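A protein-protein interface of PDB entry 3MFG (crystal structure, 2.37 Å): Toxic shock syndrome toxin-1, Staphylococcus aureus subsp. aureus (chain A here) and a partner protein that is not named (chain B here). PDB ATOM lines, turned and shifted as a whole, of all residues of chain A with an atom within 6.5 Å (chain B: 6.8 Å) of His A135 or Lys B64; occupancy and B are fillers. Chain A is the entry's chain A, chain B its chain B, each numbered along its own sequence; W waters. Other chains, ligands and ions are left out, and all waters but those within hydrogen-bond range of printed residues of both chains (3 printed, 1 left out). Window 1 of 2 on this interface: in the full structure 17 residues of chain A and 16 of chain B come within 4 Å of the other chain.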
ATOM      1  N   TRP A  12     -14.577  20.051 -13.485  1.00  0.00           N
ATOM      2  CA  TRP A  12     -15.874  19.999 -12.910  1.00  0.00           C
ATOM      3  C   TRP A  12     -16.441  18.619 -13.144  1.00  0.00           C
ATOM      4  O   TRP A  12     -16.818  17.948 -12.192  1.00  0.00           O
ATOM      5  CB  TRP A  12     -16.785  21.044 -13.558  1.00  0.00           C
ATOM      6  CG  TRP A  12     -18.194  21.118 -12.967  1.00  0.00           C
ATOM      7  CD1 TRP A  12     -19.303  20.540 -13.453  1.00  0.00           C
ATOM      8  CD2 TRP A  12     -18.582  21.813 -11.777  1.00  0.00           C
ATOM      9  NE1 TRP A  12     -20.382  20.859 -12.671  1.00  0.00           N
ATOM     10  CE2 TRP A  12     -19.951  21.646 -11.633  1.00  0.00           C
ATOM     11  CE3 TRP A  12     -17.885  22.565 -10.830  1.00  0.00           C
ATOM     12  CZ2 TRP A  12     -20.659  22.162 -10.559  1.00  0.00           C
ATOM     13  CZ3 TRP A  12     -18.593  23.121  -9.774  1.00  0.00           C
ATOM     14  CH2 TRP A  12     -19.976  22.909  -9.659  1.00  0.00           C
ATOM     15  N   TYR A  13     -16.504  18.176 -14.392  1.00  0.00           N
ATOM     16  CA  TYR A  13     -17.257  16.971 -14.640  1.00  0.00           C
ATOM     17  C   TYR A  13     -16.468  15.677 -14.447  1.00  0.00           C
ATOM     18  O   TYR A  13     -17.085  14.601 -14.376  1.00  0.00           O
ATOM     19  CB  TYR A  13     -17.859  16.964 -16.024  1.00  0.00           C
ATOM     20  CG  TYR A  13     -18.977  17.876 -16.167  1.00  0.00           C
ATOM     21  CD1 TYR A  13     -20.211  17.531 -15.709  1.00  0.00           C
ATOM     22  CD2 TYR A  13     -18.835  19.102 -16.846  1.00  0.00           C
ATOM     23  CE1 TYR A  13     -21.295  18.401 -15.857  1.00  0.00           C
ATOM     24  CE2 TYR A  13     -19.912  19.982 -16.996  1.00  0.00           C
ATOM     25  CZ  TYR A  13     -21.152  19.610 -16.519  1.00  0.00           C
ATOM     26  OH  TYR A  13     -22.264  20.429 -16.672  1.00  0.00           O
ATOM     27  N   SER A  14     -15.149  15.752 -14.388  1.00  0.00           N
ATOM     28  CA  SER A  14     -14.419  14.533 -14.005  1.00  0.00           C
ATOM     29  C   SER A  14     -14.129  14.389 -12.516  1.00  0.00           C
ATOM     30  O   SER A  14     -13.507  13.410 -12.108  1.00  0.00           O
ATOM     31  CB  SER A  14     -13.091  14.426 -14.740  1.00  0.00           C
ATOM     32  OG  SER A  14     -12.235  15.325 -14.139  1.00  0.00           O
ATOM     33  N   SER A  15     -14.559  15.332 -11.689  1.00  0.00           N
ATOM     34  CA  SER A  15     -14.313  15.181 -10.271  1.00  0.00           C
ATOM     35  C   SER A  15     -15.495  14.461  -9.641  1.00  0.00           C
ATOM     36  O   SER A  15     -16.502  14.222 -10.299  1.00  0.00           O
ATOM     37  CB  SER A  15     -14.116  16.520  -9.666  1.00  0.00           C
ATOM     38  OG  SER A  15     -15.334  17.212  -9.852  1.00  0.00           O
ATOM     39  N   GLY A  16     -15.386  14.097  -8.366  1.00  0.00           N
ATOM     40  CA  GLY A  16     -16.506  13.420  -7.699  1.00  0.00           C
ATOM     41  C   GLY A  16     -17.642  14.364  -7.316  1.00  0.00           C
ATOM     42  O   GLY A  16     -17.480  15.573  -7.384  1.00  0.00           O
ATOM     43  N   SER A  17     -18.769  13.781  -6.902  1.00  0.00           N
ATOM     44  CA  SER A  17     -19.938  14.471  -6.394  1.00  0.00           C
ATOM     45  C   SER A  17     -20.292  13.971  -4.977  1.00  0.00           C
ATOM     46  O   SER A  17     -19.897  12.894  -4.592  1.00  0.00           O
ATOM     47  CB  SER A  17     -21.111  14.123  -7.264  1.00  0.00           C
ATOM     48  OG  SER A  17     -21.314  12.709  -7.339  1.00  0.00           O
ATOM     49  N   ASP A  18     -21.096  14.736  -4.235  1.00  0.00           N
ATOM     50  CA  ASP A  18     -21.516  14.342  -2.916  1.00  0.00           C
ATOM     51  C   ASP A  18     -22.843  13.724  -3.052  1.00  0.00           C
ATOM     52  O   ASP A  18     -23.739  14.351  -3.632  1.00  0.00           O
ATOM     53  CB  ASP A  18     -21.636  15.537  -2.001  1.00  0.00           C
ATOM     54  CG  ASP A  18     -20.359  16.147  -1.675  1.00  0.00           C
ATOM     55  OD1 ASP A  18     -19.401  15.397  -1.393  1.00  0.00           O
ATOM     56  OD2 ASP A  18     -20.298  17.397  -1.633  1.00  0.00           O
ATOM     57  N   THR A  19     -23.001  12.518  -2.527  1.00  0.00           N
ATOM     58  CA  THR A  19     -24.226  11.787  -2.568  1.00  0.00           C
ATOM     59  C   THR A  19     -24.611  11.568  -1.100  1.00  0.00           C
ATOM     60  O   THR A  19     -23.954  10.843  -0.419  1.00  0.00           O
ATOM     61  CB  THR A  19     -24.027  10.479  -3.287  1.00  0.00           C
ATOM     62  OG1 THR A  19     -23.711  10.750  -4.661  1.00  0.00           O
ATOM     63  CG2 THR A  19     -25.302   9.592  -3.294  1.00  0.00           C
ATOM     64  N   LYS A  67     -22.899  18.992  -6.297  1.00  0.00           N
ATOM     65  CA  LYS A  67     -21.488  19.314  -6.486  1.00  0.00           C
ATOM     66  C   LYS A  67     -21.155  20.539  -5.709  1.00  0.00           C
ATOM     67  O   LYS A  67     -22.060  21.343  -5.417  1.00  0.00           O
ATOM     68  CB  LYS A  67     -21.175  19.564  -7.932  1.00  0.00           C
ATOM     69  CG  LYS A  67     -21.523  18.316  -8.774  1.00  0.00           C
ATOM     70  CD  LYS A  67     -20.533  17.861  -9.866  1.00  0.00           C
ATOM     71  CE  LYS A  67     -19.115  18.218  -9.754  1.00  0.00           C
ATOM     72  NZ  LYS A  67     -18.271  17.031 -10.108  1.00  0.00           N
ATOM     73  N   TRP A 116     -21.431   2.503 -16.009  1.00  0.00           N
ATOM     74  CA  TRP A 116     -22.581   3.344 -16.017  1.00  0.00           C
ATOM     75  C   TRP A 116     -23.529   2.771 -14.958  1.00  0.00           C
ATOM     76  O   TRP A 116     -24.123   1.703 -15.161  1.00  0.00           O
ATOM     77  CB  TRP A 116     -23.228   3.333 -17.411  1.00  0.00           C
ATOM     78  CG  TRP A 116     -24.580   4.089 -17.521  1.00  0.00           C
ATOM     79  CD1 TRP A 116     -25.802   3.541 -17.818  1.00  0.00           C
ATOM     80  CD2 TRP A 116     -24.802   5.484 -17.368  1.00  0.00           C
ATOM     81  NE1 TRP A 116     -26.737   4.505 -17.877  1.00  0.00           N
ATOM     82  CE2 TRP A 116     -26.163   5.709 -17.595  1.00  0.00           C
ATOM     83  CE3 TRP A 116     -23.983   6.565 -17.024  1.00  0.00           C
ATOM     84  CZ2 TRP A 116     -26.751   6.959 -17.461  1.00  0.00           C
ATOM     85  CZ3 TRP A 116     -24.558   7.842 -16.937  1.00  0.00           C
ATOM     86  CH2 TRP A 116     -25.936   8.020 -17.160  1.00  0.00           C
ATOM     87  N   ASP A 130     -27.304  15.677 -15.600  1.00  0.00           N
ATOM     88  CA  ASP A 130     -26.214  16.283 -16.359  1.00  0.00           C
ATOM     89  C   ASP A 130     -24.896  15.744 -15.918  1.00  0.00           C
ATOM     90  O   ASP A 130     -24.140  15.297 -16.761  1.00  0.00           O
ATOM     91  CB  ASP A 130     -26.179  17.770 -16.180  1.00  0.00           C
ATOM     92  CG  ASP A 130     -25.137  18.447 -17.020  1.00  0.00           C
ATOM     93  OD1 ASP A 130     -25.156  18.334 -18.286  1.00  0.00           O
ATOM     94  OD2 ASP A 130     -24.316  19.188 -16.406  1.00  0.00           O
ATOM     95  N   PHE A 131     -24.551  15.872 -14.636  1.00  0.00           N
ATOM     96  CA  PHE A 131     -23.196  15.563 -14.244  1.00  0.00           C
ATOM     97  C   PHE A 131     -22.831  14.076 -14.337  1.00  0.00           C
ATOM     98  O   PHE A 131     -21.680  13.776 -14.588  1.00  0.00           O
ATOM     99  CB  PHE A 131     -22.700  16.295 -12.966  1.00  0.00           C
ATOM    100  CG  PHE A 131     -23.281  15.816 -11.640  1.00  0.00           C
ATOM    101  CD1 PHE A 131     -22.971  14.574 -11.116  1.00  0.00           C
ATOM    102  CD2 PHE A 131     -24.018  16.711 -10.837  1.00  0.00           C
ATOM    103  CE1 PHE A 131     -23.447  14.181  -9.838  1.00  0.00           C
ATOM    104  CE2 PHE A 131     -24.488  16.334  -9.565  1.00  0.00           C
ATOM    105  CZ  PHE A 131     -24.191  15.045  -9.064  1.00  0.00           C
ATOM    106  N   GLU A 132     -23.818  13.189 -14.242  1.00  0.00           N
ATOM    107  CA  GLU A 132     -23.612  11.803 -14.354  1.00  0.00           C
ATOM    108  C   GLU A 132     -23.480  11.389 -15.826  1.00  0.00           C
ATOM    109  O   GLU A 132     -22.538  10.659 -16.200  1.00  0.00           O
ATOM    110  CB  GLU A 132     -24.796  11.079 -13.729  1.00  0.00           C
ATOM    111  CG  GLU A 132     -24.856  11.172 -12.189  1.00  0.00           C
ATOM    112  CD  GLU A 132     -23.787  10.316 -11.522  1.00  0.00           C
ATOM    113  OE1 GLU A 132     -23.302   9.414 -12.185  1.00  0.00           O
ATOM    114  OE2 GLU A 132     -23.426  10.521 -10.350  1.00  0.00           O
ATOM    115  N   ILE A 133     -24.395  11.854 -16.684  1.00  0.00           N
ATOM    116  CA  ILE A 133     -24.186  11.677 -18.123  1.00  0.00           C
ATOM    117  C   ILE A 133     -22.817  12.207 -18.508  1.00  0.00           C
ATOM    118  O   ILE A 133     -22.049  11.478 -19.114  1.00  0.00           O
ATOM    119  CB  ILE A 133     -25.211  12.357 -18.993  1.00  0.00           C
ATOM    120  CG1 ILE A 133     -26.545  11.684 -18.817  1.00  0.00           C
ATOM    121  CG2 ILE A 133     -24.773  12.276 -20.504  1.00  0.00           C
ATOM    122  CD1 ILE A 133     -27.787  12.668 -18.978  1.00  0.00           C
ATOM    123  N   ARG A 134     -22.463  13.430 -18.135  1.00  0.00           N
ATOM    124  CA  ARG A 134     -21.166  13.888 -18.591  1.00  0.00           C
ATOM    125  C   ARG A 134     -20.015  13.158 -17.958  1.00  0.00           C
ATOM    126  O   ARG A 134     -18.957  13.111 -18.573  1.00  0.00           O
ATOM    127  CB  ARG A 134     -20.961  15.364 -18.407  1.00  0.00           C
ATOM    128  CG  ARG A 134     -22.010  16.175 -19.218  1.00  0.00           C
ATOM    129  CD  ARG A 134     -21.547  17.558 -19.442  1.00  0.00           C
ATOM    130  NE  ARG A 134     -22.649  18.504 -19.507  1.00  0.00           N
ATOM    131  CZ  ARG A 134     -22.510  19.791 -19.861  1.00  0.00           C
ATOM    132  NH1 ARG A 134     -21.301  20.321 -20.175  1.00  0.00           N
ATOM    133  NH2 ARG A 134     -23.589  20.561 -19.879  1.00  0.00           N
ATOM    134  N   HIS A 135     -20.193  12.596 -16.742  1.00  0.00           N
ATOM    135  CA  HIS A 135     -19.099  11.861 -16.104  1.00  0.00           C
ATOM    136  C   HIS A 135     -18.808  10.612 -16.938  1.00  0.00           C
ATOM    137  O   HIS A 135     -17.678  10.291 -17.223  1.00  0.00           O
ATOM    138  CB  HIS A 135     -19.387  11.416 -14.678  1.00  0.00           C
ATOM    139  CG  HIS A 135     -18.158  10.980 -13.950  1.00  0.00           C
ATOM    140  ND1 HIS A 135     -17.128  11.849 -13.691  1.00  0.00           N
ATOM    141  CD2 HIS A 135     -17.782   9.787 -13.424  1.00  0.00           C
ATOM    142  CE1 HIS A 135     -16.190  11.234 -12.999  1.00  0.00           C
ATOM    143  NE2 HIS A 135     -16.583   9.996 -12.777  1.00  0.00           N
ATOM    144  N   GLN A 136     -19.852   9.954 -17.350  1.00  0.00           N
ATOM    145  CA  GLN A 136     -19.658   8.837 -18.236  1.00  0.00           C
ATOM    146  C   GLN A 136     -18.857   9.252 -19.442  1.00  0.00           C
ATOM    147  O   GLN A 136     -17.905   8.562 -19.810  1.00  0.00           O
ATOM    148  CB  GLN A 136     -20.958   8.238 -18.659  1.00  0.00           C
ATOM    149  CG  GLN A 136     -20.783   7.240 -19.818  1.00  0.00           C
ATOM    150  CD  GLN A 136     -20.276   5.846 -19.414  1.00  0.00           C
ATOM    151  OE1 GLN A 136     -20.108   5.003 -20.283  1.00  0.00           O
ATOM    152  NE2 GLN A 136     -20.065   5.595 -18.110  1.00  0.00           N
ATOM    153  N   LEU A 137     -19.174  10.430 -20.008  1.00  0.00           N
ATOM    154  CA  LEU A 137     -18.503  10.880 -21.228  1.00  0.00           C
ATOM    155  C   LEU A 137     -17.076  11.250 -20.999  1.00  0.00           C
ATOM    156  O   LEU A 137     -16.222  10.866 -21.830  1.00  0.00           O
ATOM    157  CB  LEU A 137     -19.213  12.079 -21.865  1.00  0.00           C
ATOM    158  CG  LEU A 137     -20.685  11.896 -22.292  1.00  0.00           C
ATOM    159  CD1 LEU A 137     -21.184  13.261 -22.847  1.00  0.00           C
ATOM    160  CD2 LEU A 137     -20.856  10.776 -23.268  1.00  0.00           C
ATOM    161  N   THR A 138     -16.778  12.023 -19.952  1.00  0.00           N
ATOM    162  CA  THR A 138     -15.400  12.400 -19.711  1.00  0.00           C
ATOM    163  C   THR A 138     -14.472  11.246 -19.297  1.00  0.00           C
ATOM    164  O   THR A 138     -13.289  11.313 -19.496  1.00  0.00           O
ATOM    165  CB  THR A 138     -15.278  13.393 -18.612  1.00  0.00           C
ATOM    166  OG1 THR A 138     -15.801  12.838 -17.389  1.00  0.00           O
ATOM    167  CG2 THR A 138     -16.046  14.643 -19.002  1.00  0.00           C
ATOM    168  N   GLN A 139     -15.016  10.194 -18.709  1.00  0.00           N
ATOM    169  CA  GLN A 139     -14.189   9.156 -18.093  1.00  0.00           C
ATOM    170  C   GLN A 139     -13.970   7.990 -19.053  1.00  0.00           C
ATOM    171  O   GLN A 139     -12.939   7.384 -19.061  1.00  0.00           O
ATOM    172  CB  GLN A 139     -14.872   8.622 -16.825  1.00  0.00           C
ATOM    173  CG  GLN A 139     -14.838   9.559 -15.595  1.00  0.00           C
ATOM    174  CD  GLN A 139     -13.650  10.495 -15.548  1.00  0.00           C
ATOM    175  OE1 GLN A 139     -13.692  11.603 -16.131  1.00  0.00           O
ATOM    176  NE2 GLN A 139     -12.608  10.103 -14.810  1.00  0.00           N
ATOM    177  N   ILE A 140     -14.993   7.654 -19.822  1.00  0.00           N
ATOM    178  CA  ILE A 140     -14.971   6.508 -20.682  1.00  0.00           C
ATOM    179  C   ILE A 140     -14.872   6.813 -22.164  1.00  0.00           C
ATOM    180  O   ILE A 140     -14.497   5.947 -22.932  1.00  0.00           O
ATOM    181  CB  ILE A 140     -16.238   5.752 -20.506  1.00  0.00           C
ATOM    182  CG1 ILE A 140     -16.340   5.297 -19.038  1.00  0.00           C
ATOM    183  CG2 ILE A 140     -16.307   4.576 -21.549  1.00  0.00           C
ATOM    184  CD1 ILE A 140     -15.075   4.572 -18.506  1.00  0.00           C
ATOM    185  N   HIS A 141     -15.261   8.020 -22.582  1.00  0.00           N
ATOM    186  CA  HIS A 141     -15.373   8.346 -24.003  1.00  0.00           C
ATOM    187  C   HIS A 141     -14.595   9.559 -24.437  1.00  0.00           C
ATOM    188  O   HIS A 141     -14.773   9.966 -25.545  1.00  0.00           O
ATOM    189  CB  HIS A 141     -16.821   8.549 -24.374  1.00  0.00           C
ATOM    190  CG  HIS A 141     -17.717   7.449 -23.920  1.00  0.00           C
ATOM    191  ND1 HIS A 141     -18.071   6.395 -24.731  1.00  0.00           N
ATOM    192  CD2 HIS A 141     -18.365   7.247 -22.747  1.00  0.00           C
ATOM    193  CE1 HIS A 141     -18.880   5.582 -24.074  1.00  0.00           C
ATOM    194  NE2 HIS A 141     -19.093   6.086 -22.872  1.00  0.00           N
ATOM    195  N   ALA B  56     -12.369  14.600  -5.210  1.00  0.00           N
ATOM    196  CA  ALA B  56     -11.196  14.187  -5.931  1.00  0.00           C
ATOM    197  C   ALA B  56     -11.399  14.444  -7.428  1.00  0.00           C
ATOM    198  O   ALA B  56     -12.520  14.433  -7.885  1.00  0.00           O
ATOM    199  CB  ALA B  56     -10.972  12.712  -5.689  1.00  0.00           C
ATOM    200  N   TYR B  58     -10.754  12.642 -11.082  1.00  0.00           N
ATOM    201  CA  TYR B  58     -10.461  11.327 -11.595  1.00  0.00           C
ATOM    202  C   TYR B  58      -9.946  11.303 -13.019  1.00  0.00           C
ATOM    203  O   TYR B  58     -10.512  11.940 -13.943  1.00  0.00           O
ATOM    204  CB  TYR B  58     -11.729  10.482 -11.555  1.00  0.00           C
ATOM    205  CG  TYR B  58     -12.218  10.270 -10.151  1.00  0.00           C
ATOM    206  CD1 TYR B  58     -13.115  11.134  -9.569  1.00  0.00           C
ATOM    207  CD2 TYR B  58     -11.760   9.188  -9.404  1.00  0.00           C
ATOM    208  CE1 TYR B  58     -13.561  10.930  -8.272  1.00  0.00           C
ATOM    209  CE2 TYR B  58     -12.168   8.978  -8.145  1.00  0.00           C
ATOM    210  CZ  TYR B  58     -13.067   9.859  -7.566  1.00  0.00           C
ATOM    211  OH  TYR B  58     -13.487   9.610  -6.309  1.00  0.00           O
ATOM    212  N   VAL B  62     -11.459   5.927 -14.810  1.00  0.00           N
ATOM    213  CA  VAL B  62     -11.870   5.759 -13.434  1.00  0.00           C
ATOM    214  C   VAL B  62     -13.169   6.515 -13.133  1.00  0.00           C
ATOM    215  O   VAL B  62     -13.229   7.725 -13.294  1.00  0.00           O
ATOM    216  CB  VAL B  62     -10.801   6.299 -12.517  1.00  0.00           C
ATOM    217  CG1 VAL B  62     -11.179   6.075 -11.050  1.00  0.00           C
ATOM    218  CG2 VAL B  62      -9.432   5.703 -12.898  1.00  0.00           C
ATOM    219  N   GLU B  63     -14.183   5.762 -12.680  1.00  0.00           N
ATOM    220  CA  GLU B  63     -15.505   6.237 -12.344  1.00  0.00           C
ATOM    221  C   GLU B  63     -15.624   6.626 -10.869  1.00  0.00           C
ATOM    222  O   GLU B  63     -15.273   5.840  -9.951  1.00  0.00           O
ATOM    223  CB  GLU B  63     -16.530   5.128 -12.620  1.00  0.00           C
ATOM    224  CG  GLU B  63     -17.852   5.674 -13.141  1.00  0.00           C
ATOM    225  CD  GLU B  63     -18.815   6.134 -12.048  1.00  0.00           C
ATOM    226  OE1 GLU B  63     -18.578   5.753 -10.879  1.00  0.00           O
ATOM    227  OE2 GLU B  63     -19.818   6.862 -12.350  1.00  0.00           O
ATOM    228  N   LYS B  64     -16.147   7.799 -10.634  1.00  0.00           N
ATOM    229  CA  LYS B  64     -16.087   8.423  -9.302  1.00  0.00           C
ATOM    230  C   LYS B  64     -16.747   7.596  -8.175  1.00  0.00           C
ATOM    231  O   LYS B  64     -16.326   7.633  -7.038  1.00  0.00           O
ATOM    232  CB  LYS B  64     -16.745   9.817  -9.338  1.00  0.00           C
ATOM    233  CG  LYS B  64     -18.216   9.783  -9.656  1.00  0.00           C
ATOM    234  CD  LYS B  64     -18.789  11.191 -10.019  1.00  0.00           C
ATOM    235  CE  LYS B  64     -20.254  11.097 -10.403  1.00  0.00           C
ATOM    236  NZ  LYS B  64     -21.245  10.917  -9.280  1.00  0.00           N
ATOM    237  N   ASP B  65     -17.806   6.905  -8.489  1.00  0.00           N
ATOM    238  CA  ASP B  65     -18.564   6.227  -7.473  1.00  0.00           C
ATOM    239  C   ASP B  65     -18.083   4.813  -7.243  1.00  0.00           C
ATOM    240  O   ASP B  65     -18.554   4.189  -6.274  1.00  0.00           O
ATOM    241  CB  ASP B  65     -20.060   6.182  -7.844  1.00  0.00           C
ATOM    242  CG  ASP B  65     -20.789   7.498  -7.526  1.00  0.00           C
ATOM    243  OD1 ASP B  65     -21.998   7.522  -7.784  1.00  0.00           O
ATOM    244  OD2 ASP B  65     -20.181   8.501  -7.064  1.00  0.00           O
ATOM    245  N   LYS B  66     -17.240   4.291  -8.163  1.00  0.00           N
ATOM    246  CA  LYS B  66     -16.492   3.066  -7.897  1.00  0.00           C
ATOM    247  C   LYS B  66     -15.334   3.289  -6.942  1.00  0.00           C
ATOM    248  O   LYS B  66     -14.911   2.346  -6.321  1.00  0.00           O
ATOM    249  CB  LYS B  66     -15.957   2.468  -9.183  1.00  0.00           C
ATOM    250  CG  LYS B  66     -16.963   1.587  -9.928  1.00  0.00           C
ATOM    251  CD  LYS B  66     -16.244   0.680 -10.958  1.00  0.00           C
ATOM    252  CE  LYS B  66     -15.129  -0.268 -10.401  1.00  0.00           C
ATOM    253  NZ  LYS B  66     -15.575  -1.387  -9.501  1.00  0.00           N
ATOM    254  N   PHE B  67     -14.826   4.518  -6.830  1.00  0.00           N
ATOM    255  CA  PHE B  67     -13.629   4.829  -6.085  1.00  0.00           C
ATOM    256  C   PHE B  67     -13.760   6.068  -5.274  1.00  0.00           C
ATOM    257  O   PHE B  67     -13.050   7.059  -5.501  1.00  0.00           O
ATOM    258  CB  PHE B  67     -12.391   4.926  -6.978  1.00  0.00           C
ATOM    259  CG  PHE B  67     -12.049   3.654  -7.662  1.00  0.00           C
ATOM    260  CD1 PHE B  67     -11.235   2.704  -7.037  1.00  0.00           C
ATOM    261  CD2 PHE B  67     -12.533   3.358  -8.908  1.00  0.00           C
ATOM    262  CE1 PHE B  67     -10.916   1.444  -7.672  1.00  0.00           C
ATOM    263  CE2 PHE B  67     -12.210   2.120  -9.570  1.00  0.00           C
ATOM    264  CZ  PHE B  67     -11.408   1.183  -8.941  1.00  0.00           C
ATOM    265  N   LEU B  68     -14.627   6.008  -4.281  1.00  0.00           N
ATOM    266  CA  LEU B  68     -14.871   7.153  -3.442  1.00  0.00           C
ATOM    267  C   LEU B  68     -13.613   7.575  -2.783  1.00  0.00           C
ATOM    268  O   LEU B  68     -12.811   6.728  -2.407  1.00  0.00           O
ATOM    269  CB  LEU B  68     -15.925   6.827  -2.358  1.00  0.00           C
ATOM    270  CG  LEU B  68     -17.319   6.446  -2.913  1.00  0.00           C
ATOM    271  CD1 LEU B  68     -18.364   6.109  -1.808  1.00  0.00           C
ATOM    272  CD2 LEU B  68     -17.865   7.589  -3.857  1.00  0.00           C
ATOM    273  N   ILE B  69     -13.443   8.862  -2.562  1.00  0.00           N
ATOM    274  CA  ILE B  69     -12.308   9.383  -1.852  1.00  0.00           C
ATOM    275  C   ILE B  69     -12.831  10.372  -0.886  1.00  0.00           C
ATOM    276  O   ILE B  69     -13.596  11.237  -1.263  1.00  0.00           O
ATOM    277  CB  ILE B  69     -11.283  10.011  -2.814  1.00  0.00           C
ATOM    278  CG1 ILE B  69     -10.559   8.894  -3.582  1.00  0.00           C
ATOM    279  CG2 ILE B  69     -10.244  10.825  -2.068  1.00  0.00           C
ATOM    280  CD1 ILE B  69      -9.720   9.317  -4.766  1.00  0.00           C
ATOM    281  N   THR B  80     -12.336   4.244  -1.031  1.00  0.00           N
ATOM    282  CA  THR B  80     -13.177   3.086  -0.789  1.00  0.00           C
ATOM    283  C   THR B  80     -13.588   2.502  -2.087  1.00  0.00           C
ATOM    284  O   THR B  80     -14.234   3.155  -2.837  1.00  0.00           O
ATOM    285  CB  THR B  80     -14.317   3.318   0.330  1.00  0.00           C
ATOM    286  OG1 THR B  80     -15.591   2.874  -0.152  1.00  0.00           O
ATOM    287  CG2 THR B  80     -14.459   4.614   0.721  1.00  0.00           C
ATOM    288  N   THR B  82     -16.008   0.624  -3.739  1.00  0.00           N
ATOM    289  CA  THR B  82     -17.355   0.266  -3.367  1.00  0.00           C
ATOM    290  C   THR B  82     -17.766  -0.938  -4.225  1.00  0.00           C
ATOM    291  O   THR B  82     -17.291  -1.072  -5.361  1.00  0.00           O
ATOM    292  CB  THR B  82     -18.270   1.464  -3.626  1.00  0.00           C
ATOM    293  OG1 THR B  82     -18.289   1.711  -5.023  1.00  0.00           O
ATOM    294  CG2 THR B  82     -17.752   2.695  -2.911  1.00  0.00           C
HETATM  295  O   HOH W   1     -20.557   6.479 -15.629  1.00  0.00           O
HETATM  296  O   HOH W   2     -18.738  10.561  -6.307  1.00  0.00           O
HETATM  297  O   HOH W   3     -24.139   8.897  -6.735  1.00  0.00           O
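Among the printed residues, merely in contact across the chains: Ser A15 with Ala B56, Gly A16 with Tyr B58, His A135 with Glu B63, Ser A15 with Lys B64, Gly A16 with Lys B64 and Phe A131 with Lys B64.
Water W2 lies within hydrogen-bond range of OD2 of Asp B65 and O of Ser A17. Water W1 bridges NE2 of Gln A136 and OE2 of Glu B63. Water W3 bridges the side-chain carboxylate (OD1) of Asp B65 (2.8 Å) and the side-chain hydroxyl (OG1) of Thr A19 (2.8 Å).
OG1 of Thr A138 is in hydrogen-bond range of OE1 of Gln A139. The backbone carbonyl oxygen (O) of Tyr A13 is in hydrogen-bond range of a ring nitrogen (ND1) of His A135 (2.8 Å). OG of Ser A15 lies within hydrogen-bond range of O of Trp A12. The backbone carbonyl oxygen (O) of His A135 is in hydrogen-bond range of the side-chain hydroxyl (OG1) of Thr A138 (3.2 Å). The side-chain hydroxyl of Ser A15 is in hydrogen-bond range of the side-chain amino group of Lys A67, 3.0 Å away. OH of Tyr B58 lies within hydrogen-bond range of O of Phe B67, at 2.7 Å.
Of the 12 printed residues of chain B, 5 touch a printed residue of chain A. Of the 22 printed residues of chain A, 8 touch a printed residue of chain B. Printed residues of chain A that touch a printed residue of chain B: Ser A14, Ser A15, Gly A16, Ser A17, Phe A131, Glu A132, His A135 and Gln A139. Among the printed residues, 13 pairs touch across the chains.
The side-chain amino group (NZ) of Lys B64 is in hydrogen-bond range of the side-chain hydroxyl (OG) of Ser A17 (2.6 Å). OE2 of Glu A132 lies within salt-bridge range of NZ of Lys B64 (2.5 Å). The side-chain amide nitrogen of Gln A139 lies within hydrogen-bond range of the backbone carbonyl oxygen of Val B62 (2.9 Å). NE2 of His A135 lies within hydrogen-bond range of N of Lys B64 (3.1 Å). NE2 of Gln A139 sits at hydrogen-bond distance from O of Tyr B58 (2.9 Å). The backbone NH (N) of Gly A16 lies within hydrogen-bond range of the backbone carbonyl oxygen (O) of Ala B56, 2.9 Å away. The backbone carbonyl oxygen (O) of Ser A14 lies within hydrogen-bond range of the backbone NH (N) of Tyr B58 (3.0 Å).
Printed residues of chain B within 4 Å of Ser A14: Tyr B58. His A135 touches just these residues of chain B: Glu B63 and Lys B64. Gln A136 touches none of the printed residues of chain B. Printed residues of chain B within 4 Å of Gln A139: Tyr B58 and Val B62. Printed residues of chain A within 4 Å of Ala B56: Ser A15 (3.1 Å) and Gly A16 (2.9 Å). Of the printed residues of chain A, Val B62 touches Gln A139 (2.9 Å). Of chain A, only Ser A15, Gly A16, Ser A17, Phe A131, Glu A132 and His A135 come within 4 Å of Lys B64. The nearest residue of chain A that does not touch Lys B64 is Thr A19 (5.2 Å). The nearest printed residue of chain B that does not touch Glu A132 is Asp B65 (4.2 Å).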
